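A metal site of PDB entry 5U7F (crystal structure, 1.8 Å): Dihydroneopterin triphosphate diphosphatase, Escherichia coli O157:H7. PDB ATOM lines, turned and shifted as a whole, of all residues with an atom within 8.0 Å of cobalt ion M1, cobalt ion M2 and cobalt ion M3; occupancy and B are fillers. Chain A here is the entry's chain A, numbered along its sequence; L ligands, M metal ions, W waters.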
ATOM      1  N   LYS A   7     -15.494  -7.162  23.759  1.00  0.00           N
ATOM      2  CA  LYS A   7     -16.219  -7.713  24.888  1.00  0.00           C
ATOM      3  C   LYS A   7     -15.538  -7.286  26.210  1.00  0.00           C
ATOM      4  O   LYS A   7     -14.315  -7.137  26.256  1.00  0.00           O
ATOM      5  CB  LYS A   7     -16.261  -9.236  24.795  1.00  0.00           C
ATOM      6  CG  LYS A   7     -17.295  -9.825  23.859  1.00  0.00           C
ATOM      7  CD  LYS A   7     -17.521 -11.308  24.186  1.00  0.00           C
ATOM      8  CE  LYS A   7     -18.861 -11.797  23.633  1.00  0.00           C
ATOM      9  NZ  LYS A   7     -19.542 -12.744  24.561  1.00  0.00           N
ATOM     10  N   ILE A  12     -21.316 -12.470  33.658  1.00  0.00           N
ATOM     11  CA  ILE A  12     -22.232 -13.198  34.501  1.00  0.00           C
ATOM     12  C   ILE A  12     -22.589 -14.514  33.842  1.00  0.00           C
ATOM     13  O   ILE A  12     -22.473 -14.680  32.626  1.00  0.00           O
ATOM     14  CB  ILE A  12     -23.501 -12.368  34.835  1.00  0.00           C
ATOM     15  CG1 ILE A  12     -24.245 -11.881  33.594  1.00  0.00           C
ATOM     16  CG2 ILE A  12     -23.131 -11.162  35.697  1.00  0.00           C
ATOM     17  CD1 ILE A  12     -25.169 -12.890  32.988  1.00  0.00           C
ATOM     18  N   LEU A  27     -27.699 -24.162  25.855  1.00  0.00           N
ATOM     19  CA  LEU A  27     -27.862 -23.378  24.639  1.00  0.00           C
ATOM     20  C   LEU A  27     -26.607 -23.526  23.801  1.00  0.00           C
ATOM     21  O   LEU A  27     -25.513 -23.447  24.311  1.00  0.00           O
ATOM     22  CB  LEU A  27     -28.124 -21.914  24.989  1.00  0.00           C
ATOM     23  CG  LEU A  27     -29.259 -21.599  25.947  1.00  0.00           C
ATOM     24  CD1 LEU A  27     -29.160 -20.194  26.473  1.00  0.00           C
ATOM     25  CD2 LEU A  27     -30.555 -21.781  25.230  1.00  0.00           C
ATOM     26  N   ARG A  29     -23.873 -22.404  21.189  1.00  0.00           N
ATOM     27  CA  ARG A  29     -23.349 -21.123  20.734  1.00  0.00           C
ATOM     28  C   ARG A  29     -23.235 -21.003  19.214  1.00  0.00           C
ATOM     29  O   ARG A  29     -23.108 -22.010  18.508  1.00  0.00           O
ATOM     30  CB  ARG A  29     -21.968 -20.838  21.330  1.00  0.00           C
ATOM     31  CG  ARG A  29     -22.013 -20.533  22.795  1.00  0.00           C
ATOM     32  CD  ARG A  29     -20.651 -20.000  23.270  1.00  0.00           C
ATOM     33  NE  ARG A  29     -20.331 -18.728  22.631  1.00  0.00           N
ATOM     34  CZ  ARG A  29     -20.851 -17.559  22.998  1.00  0.00           C
ATOM     35  NH1 ARG A  29     -21.743 -17.491  23.987  1.00  0.00           N
ATOM     36  NH2 ARG A  29     -20.502 -16.438  22.369  1.00  0.00           N
ATOM     37  N   GLN A  37     -23.945 -24.122  26.618  1.00  0.00           N
ATOM     38  CA  GLN A  37     -23.788 -23.351  27.863  1.00  0.00           C
ATOM     39  C   GLN A  37     -25.106 -22.893  28.424  1.00  0.00           C
ATOM     40  O   GLN A  37     -26.115 -22.853  27.709  1.00  0.00           O
ATOM     41  CB  GLN A  37     -22.929 -22.117  27.592  1.00  0.00           C
ATOM     42  CG  GLN A  37     -23.459 -21.270  26.474  1.00  0.00           C
ATOM     43  CD  GLN A  37     -22.909 -19.863  26.433  1.00  0.00           C
ATOM     44  OE1 GLN A  37     -23.370 -19.028  25.622  1.00  0.00           O
ATOM     45  NE2 GLN A  37     -21.892 -19.593  27.239  1.00  0.00           N
ATOM     46  N   SER A  38     -25.090 -22.522  29.710  1.00  0.00           N
ATOM     47  CA  SER A  38     -26.153 -21.724  30.279  1.00  0.00           C
ATOM     48  C   SER A  38     -26.018 -20.269  29.765  1.00  0.00           C
ATOM     49  O   SER A  38     -25.170 -19.974  28.893  1.00  0.00           O
ATOM     50  CB  SER A  38     -26.101 -21.782  31.831  1.00  0.00           C
ATOM     51  OG  SER A  38     -25.853 -23.120  32.274  1.00  0.00           O
ATOM     52  N   VAL A  39     -26.883 -19.360  30.219  1.00  0.00           N
ATOM     53  CA  VAL A  39     -26.806 -17.967  29.794  1.00  0.00           C
ATOM     54  C   VAL A  39     -25.535 -17.287  30.345  1.00  0.00           C
ATOM     55  O   VAL A  39     -25.284 -17.352  31.537  1.00  0.00           O
ATOM     56  CB  VAL A  39     -28.054 -17.211  30.225  1.00  0.00           C
ATOM     57  CG1 VAL A  39     -27.903 -15.715  30.076  1.00  0.00           C
ATOM     58  CG2 VAL A  39     -29.248 -17.682  29.395  1.00  0.00           C
ATOM     59  N   THR A  40     -24.714 -16.686  29.481  1.00  0.00           N
ATOM     60  CA  THR A  40     -23.567 -15.884  29.935  1.00  0.00           C
ATOM     61  C   THR A  40     -23.637 -14.537  29.238  1.00  0.00           C
ATOM     62  O   THR A  40     -24.281 -14.417  28.194  1.00  0.00           O
ATOM     63  CB  THR A  40     -22.182 -16.538  29.653  1.00  0.00           C
ATOM     64  OG1 THR A  40     -21.938 -16.589  28.251  1.00  0.00           O
ATOM     65  CG2 THR A  40     -22.091 -17.922  30.254  1.00  0.00           C
ATOM     66  N   GLY A  41     -23.026 -13.517  29.816  1.00  0.00           N
ATOM     67  CA  GLY A  41     -22.960 -12.231  29.164  1.00  0.00           C
ATOM     68  C   GLY A  41     -22.054 -11.271  29.893  1.00  0.00           C
ATOM     69  O   GLY A  41     -21.872 -11.418  31.107  1.00  0.00           O
ATOM     70  N   SER A  42     -21.487 -10.320  29.152  1.00  0.00           N
ATOM     71  CA  SER A  42     -20.665  -9.259  29.733  1.00  0.00           C
ATOM     72  C   SER A  42     -21.480  -8.272  30.565  1.00  0.00           C
ATOM     73  O   SER A  42     -22.611  -7.939  30.227  1.00  0.00           O
ATOM     74  CB  SER A  42     -19.915  -8.470  28.638  1.00  0.00           C
ATOM     75  OG  SER A  42     -18.932  -9.269  28.001  1.00  0.00           O
ATOM     76  N   VAL A  43     -20.871  -7.832  31.680  1.00  0.00           N
ATOM     77  CA  VAL A  43     -21.389  -6.717  32.479  1.00  0.00           C
ATOM     78  C   VAL A  43     -20.943  -5.416  31.846  1.00  0.00           C
ATOM     79  O   VAL A  43     -19.748  -5.124  31.798  1.00  0.00           O
ATOM     80  CB  VAL A  43     -20.877  -6.773  33.925  1.00  0.00           C
ATOM     81  CG1 VAL A  43     -21.489  -5.650  34.763  1.00  0.00           C
ATOM     82  CG2 VAL A  43     -21.187  -8.118  34.519  1.00  0.00           C
ATOM     83  N   GLU A  44     -21.906  -4.625  31.383  1.00  0.00           N
ATOM     84  CA  GLU A  44     -21.568  -3.369  30.706  1.00  0.00           C
ATOM     85  C   GLU A  44     -21.302  -2.233  31.676  1.00  0.00           C
ATOM     86  O   GLU A  44     -21.713  -2.269  32.826  1.00  0.00           O
ATOM     87  CB  GLU A  44     -22.690  -2.962  29.750  1.00  0.00           C
ATOM     88  CG  GLU A  44     -23.002  -4.012  28.691  1.00  0.00           C
ATOM     89  CD  GLU A  44     -21.814  -4.320  27.767  1.00  0.00           C
ATOM     90  OE1 GLU A  44     -20.898  -3.478  27.666  1.00  0.00           O
ATOM     91  OE2 GLU A  44     -21.786  -5.405  27.139  1.00  0.00           O
ATOM     92  N   GLU A  47     -23.679  -0.762  34.725  1.00  0.00           N
ATOM     93  CA  GLU A  47     -24.644  -1.707  35.274  1.00  0.00           C
ATOM     94  C   GLU A  47     -23.992  -2.676  36.269  1.00  0.00           C
ATOM     95  O   GLU A  47     -22.776  -2.906  36.265  1.00  0.00           O
ATOM     96  CB  GLU A  47     -25.389  -2.481  34.137  1.00  0.00           C
ATOM     97  CG  GLU A  47     -24.627  -3.632  33.472  1.00  0.00           C
ATOM     98  CD  GLU A  47     -25.383  -4.350  32.311  1.00  0.00           C
ATOM     99  OE1 GLU A  47     -26.648  -4.340  32.264  1.00  0.00           O
ATOM    100  OE2 GLU A  47     -24.695  -4.946  31.449  1.00  0.00           O
ATOM    101  N   ALA A  52     -27.103  -7.113  34.859  1.00  0.00           N
ATOM    102  CA  ALA A  52     -26.636  -7.693  33.616  1.00  0.00           C
ATOM    103  C   ALA A  52     -27.260  -9.072  33.432  1.00  0.00           C
ATOM    104  O   ALA A  52     -27.673  -9.445  32.344  1.00  0.00           O
ATOM    105  CB  ALA A  52     -25.102  -7.771  33.610  1.00  0.00           C
ATOM    106  N   ARG A  55     -30.789  -8.751  32.395  1.00  0.00           N
ATOM    107  CA  ARG A  55     -30.859  -8.265  31.027  1.00  0.00           C
ATOM    108  C   ARG A  55     -30.560  -9.365  30.036  1.00  0.00           C
ATOM    109  O   ARG A  55     -31.285  -9.535  29.066  1.00  0.00           O
ATOM    110  CB  ARG A  55     -29.918  -7.100  30.800  1.00  0.00           C
ATOM    111  CG  ARG A  55     -29.907  -6.626  29.341  1.00  0.00           C
ATOM    112  CD  ARG A  55     -28.916  -5.567  29.080  1.00  0.00           C
ATOM    113  NE  ARG A  55     -27.630  -5.850  29.721  1.00  0.00           N
ATOM    114  CZ  ARG A  55     -26.720  -6.682  29.238  1.00  0.00           C
ATOM    115  NH1 ARG A  55     -26.915  -7.299  28.071  1.00  0.00           N
ATOM    116  NH2 ARG A  55     -25.598  -6.868  29.908  1.00  0.00           N
ATOM    117  N   GLU A  56     -29.462 -10.098  30.249  1.00  0.00           N
ATOM    118  CA  GLU A  56     -29.071 -11.177  29.360  1.00  0.00           C
ATOM    119  C   GLU A  56     -30.117 -12.297  29.325  1.00  0.00           C
ATOM    120  O   GLU A  56     -30.318 -12.943  28.314  1.00  0.00           O
ATOM    121  CB  GLU A  56     -27.721 -11.734  29.798  1.00  0.00           C
ATOM    122  CG  GLU A  56     -26.591 -10.752  29.600  1.00  0.00           C
ATOM    123  CD  GLU A  56     -26.137 -10.597  28.117  1.00  0.00           C
ATOM    124  OE1 GLU A  56     -26.483 -11.468  27.322  1.00  0.00           O
ATOM    125  OE2 GLU A  56     -25.416  -9.614  27.796  1.00  0.00           O
ATOM    126  N   VAL A  57     -30.799 -12.530  30.449  1.00  0.00           N
ATOM    127  CA  VAL A  57     -31.804 -13.581  30.466  1.00  0.00           C
ATOM    128  C   VAL A  57     -32.965 -13.150  29.569  1.00  0.00           C
ATOM    129  O   VAL A  57     -33.502 -13.964  28.803  1.00  0.00           O
ATOM    130  CB  VAL A  57     -32.281 -13.891  31.901  1.00  0.00           C
ATOM    131  CG1 VAL A  57     -33.570 -14.734  31.877  1.00  0.00           C
ATOM    132  CG2 VAL A  57     -31.161 -14.624  32.651  1.00  0.00           C
ATOM    133  N   GLU A  59     -32.741 -10.909  26.974  1.00  0.00           N
ATOM    134  CA  GLU A  59     -32.175 -10.918  25.596  1.00  0.00           C
ATOM    135  C   GLU A  59     -31.990 -12.317  24.994  1.00  0.00           C
ATOM    136  O   GLU A  59     -32.318 -12.534  23.826  1.00  0.00           O
ATOM    137  CB  GLU A  59     -30.810 -10.196  25.567  1.00  0.00           C
ATOM    138  CG  GLU A  59     -30.847  -8.678  25.803  1.00  0.00           C
ATOM    139  CD  GLU A  59     -29.452  -8.005  25.793  1.00  0.00           C
ATOM    140  OE1 GLU A  59     -29.374  -6.772  26.035  1.00  0.00           O
ATOM    141  OE2 GLU A  59     -28.442  -8.701  25.537  1.00  0.00           O
ATOM    142  N   GLU A  60     -31.446 -13.249  25.774  1.00  0.00           N
ATOM    143  CA  GLU A  60     -31.016 -14.537  25.239  1.00  0.00           C
ATOM    144  C   GLU A  60     -32.050 -15.640  25.227  1.00  0.00           C
ATOM    145  O   GLU A  60     -32.007 -16.521  24.374  1.00  0.00           O
ATOM    146  CB  GLU A  60     -29.803 -15.029  26.025  1.00  0.00           C
ATOM    147  CG  GLU A  60     -28.575 -14.087  25.824  1.00  0.00           C
ATOM    148  CD  GLU A  60     -27.239 -14.705  26.126  1.00  0.00           C
ATOM    149  OE1 GLU A  60     -27.207 -15.852  26.572  1.00  0.00           O
ATOM    150  OE2 GLU A  60     -26.196 -14.017  25.904  1.00  0.00           O
ATOM    151  N   THR A 116     -32.112 -15.972  20.900  1.00  0.00           N
ATOM    152  CA  THR A 116     -31.625 -14.961  19.964  1.00  0.00           C
ATOM    153  C   THR A 116     -30.121 -15.091  19.643  1.00  0.00           C
ATOM    154  O   THR A 116     -29.693 -14.921  18.497  1.00  0.00           O
ATOM    155  CB  THR A 116     -31.902 -13.550  20.516  1.00  0.00           C
ATOM    156  OG1 THR A 116     -31.245 -13.384  21.771  1.00  0.00           O
ATOM    157  CG2 THR A 116     -33.387 -13.342  20.723  1.00  0.00           C
ATOM    158  N   GLU A 117     -29.322 -15.414  20.651  1.00  0.00           N
ATOM    159  CA  GLU A 117     -27.876 -15.452  20.537  1.00  0.00           C
ATOM    160  C   GLU A 117     -27.332 -16.841  20.134  1.00  0.00           C
ATOM    161  O   GLU A 117     -26.145 -16.993  19.835  1.00  0.00           O
ATOM    162  CB  GLU A 117     -27.263 -15.000  21.899  1.00  0.00           C
ATOM    163  CG  GLU A 117     -25.752 -14.825  21.947  1.00  0.00           C
ATOM    164  CD  GLU A 117     -25.262 -14.264  23.306  1.00  0.00           C
ATOM    165  OE1 GLU A 117     -24.573 -15.008  24.063  1.00  0.00           O
ATOM    166  OE2 GLU A 117     -25.568 -13.078  23.609  1.00  0.00           O
ATOM    167  N   HIS A 118     -28.213 -17.849  20.097  1.00  0.00           N
ATOM    168  CA  HIS A 118     -27.777 -19.231  19.978  1.00  0.00           C
ATOM    169  C   HIS A 118     -28.387 -19.956  18.761  1.00  0.00           C
ATOM    170  O   HIS A 118     -29.193 -19.380  18.069  1.00  0.00           O
ATOM    171  CB  HIS A 118     -28.134 -19.973  21.253  1.00  0.00           C
ATOM    172  CG  HIS A 118     -27.373 -19.484  22.450  1.00  0.00           C
ATOM    173  ND1 HIS A 118     -27.756 -18.368  23.168  1.00  0.00           N
ATOM    174  CD2 HIS A 118     -26.229 -19.927  23.024  1.00  0.00           C
ATOM    175  CE1 HIS A 118     -26.903 -18.164  24.153  1.00  0.00           C
ATOM    176  NE2 HIS A 118     -25.968 -19.098  24.100  1.00  0.00           N
HETATM  177  S1  LIG L   1     -22.513 -11.895  25.585  1.00  0.00           S
HETATM  178  O1  LIG L   1     -21.343 -12.661  26.047  1.00  0.00           O
HETATM  179  O2  LIG L   1     -22.369 -11.665  24.144  1.00  0.00           O
HETATM  180  O3  LIG L   1     -23.750 -12.657  25.882  1.00  0.00           O
HETATM  181  O4  LIG L   1     -22.563 -10.606  26.266  1.00  0.00           O
HETATM  182 CO    CO M   1     -25.811 -12.010  25.446  1.00  0.00          CO
HETATM  183 CO    CO M   2     -24.142  -9.095  26.173  1.00  0.00          CO
HETATM  184 CO    CO M   3     -24.244 -14.677  26.159  1.00  0.00          CO
HETATM  185 CO    CO M   4     -23.586 -10.042  23.367  1.00  0.00          CO
HETATM  186  O   HOH W   1     -23.158  -7.764  27.519  1.00  0.00           O
HETATM  187  O   HOH W   2     -24.773 -16.742  26.659  1.00  0.00           O
HETATM  188  O   HOH W   3     -22.075 -14.898  26.194  1.00  0.00           O
HETATM  189  O   HOH W   4     -22.858  -8.328  24.447  1.00  0.00           O
HETATM  190  O   HOH W   5     -27.668 -11.277  24.663  1.00  0.00           O
HETATM  191  O   HOH W   6     -25.259 -10.239  24.944  1.00  0.00           O
HETATM  192  O   HOH W   7     -25.627  -7.637  25.575  1.00  0.00           O
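The guanidinium group (NH2) of Arg 55 is in hydrogen-bond range of the backbone carbonyl oxygen (O) of Ser 42.
NE2 of Gln 37 lies within hydrogen-bond range of OG1 of Thr 40.
OE2 of Glu 47 lies within salt-bridge range of NH2 of Arg 55 (2.6 Å).
OE1 of Glu 117 sits close to NH1 of Arg 29 (3.8 Å).
The side-chain carboxylate of Glu 59 lies within salt-bridge range of the guanidinium group of Arg 55 (3.2 Å).
The side-chain carboxylate (OE2) of Glu 56 lies close to the guanidinium group (NH1) of Arg 55, 2.8 Å away.
Within 4 Å of cobalt ion M1: Thr 40, Glu 56, Glu 60 and Glu 117.
The nearest printed residue that does not touch cobalt ion M1 is Glu 59 (4.2 Å).
Arg 55 touches cobalt ion M2 (NH1 to CO, 3.8 Å).
Of the 22 residues printed, 2 come within 4 Å of cobalt ion M2.
Within 4 Å of cobalt ion M3: Thr 40, Glu 60 and Glu 117.
The nearest printed residue that does not touch cobalt ion M3 is Gly 41 (4.03 Å).
Cobalt ion M1 is bound by water W6 (1.9 Å), the side-chain carboxylate of Glu 56 (2.1 Å), the side-chain carboxylate of Glu 60 (2.1 Å), the side-chain carboxylate of Glu 117 (2.1 Å), water W5 (2.1 Å) and an oxygen (O3) of the ligand (2.2 Å).
Water W6 is bound to cobalt ion M2 (2.0 Å).
The side-chain carboxylate (OE2) of Glu 56 binds cobalt ion M2 (2.1 Å).
Cobalt ion M2 is bound by water W1 (2.1 Å).
Cobalt ion M2 is bound by water W7 (2.2 Å).
Cobalt ion M2 is bound by an oxygen (O4) of the ligand, 2.2 Å away.
Water W4 is bound to cobalt ion M2.
Cobalt ion M2 has six donor atoms within binding distance.
The backbone carbonyl oxygen (O) of Thr 40 is bound to cobalt ion M3 (2.1 Å).
OE2 of Glu 60 binds cobalt ion M3 (2.1 Å).
O3 of the ligand is bound to cobalt ion M3 (2.1 Å).
Cobalt ion M3 is bound by OE1 of Glu 117, at 2.1 Å.
Water W3 binds cobalt ion M3, 2.2 Å away.
Water W2 is bound to cobalt ion M3.
Cobalt ion M3 has six donor atoms within binding distance.
Water W7 lies within hydrogen-bond range of the guanidinium group of Arg 55 (2.8 Å) and the side-chain carboxylate of Glu 59 (3.0 Å).
Water W1 bridges OE2 of Glu 44 (2.8 Å) and O of Ser 42 (2.8 Å).
Water W3 bridges OG1 of Thr 40 and NH1 of Arg 29.
Water W2 lies within hydrogen-bond range of the side-chain carboxylate of Glu 60, the backbone NH of Thr 40 and the side-chain amide oxygen of Gln 37.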
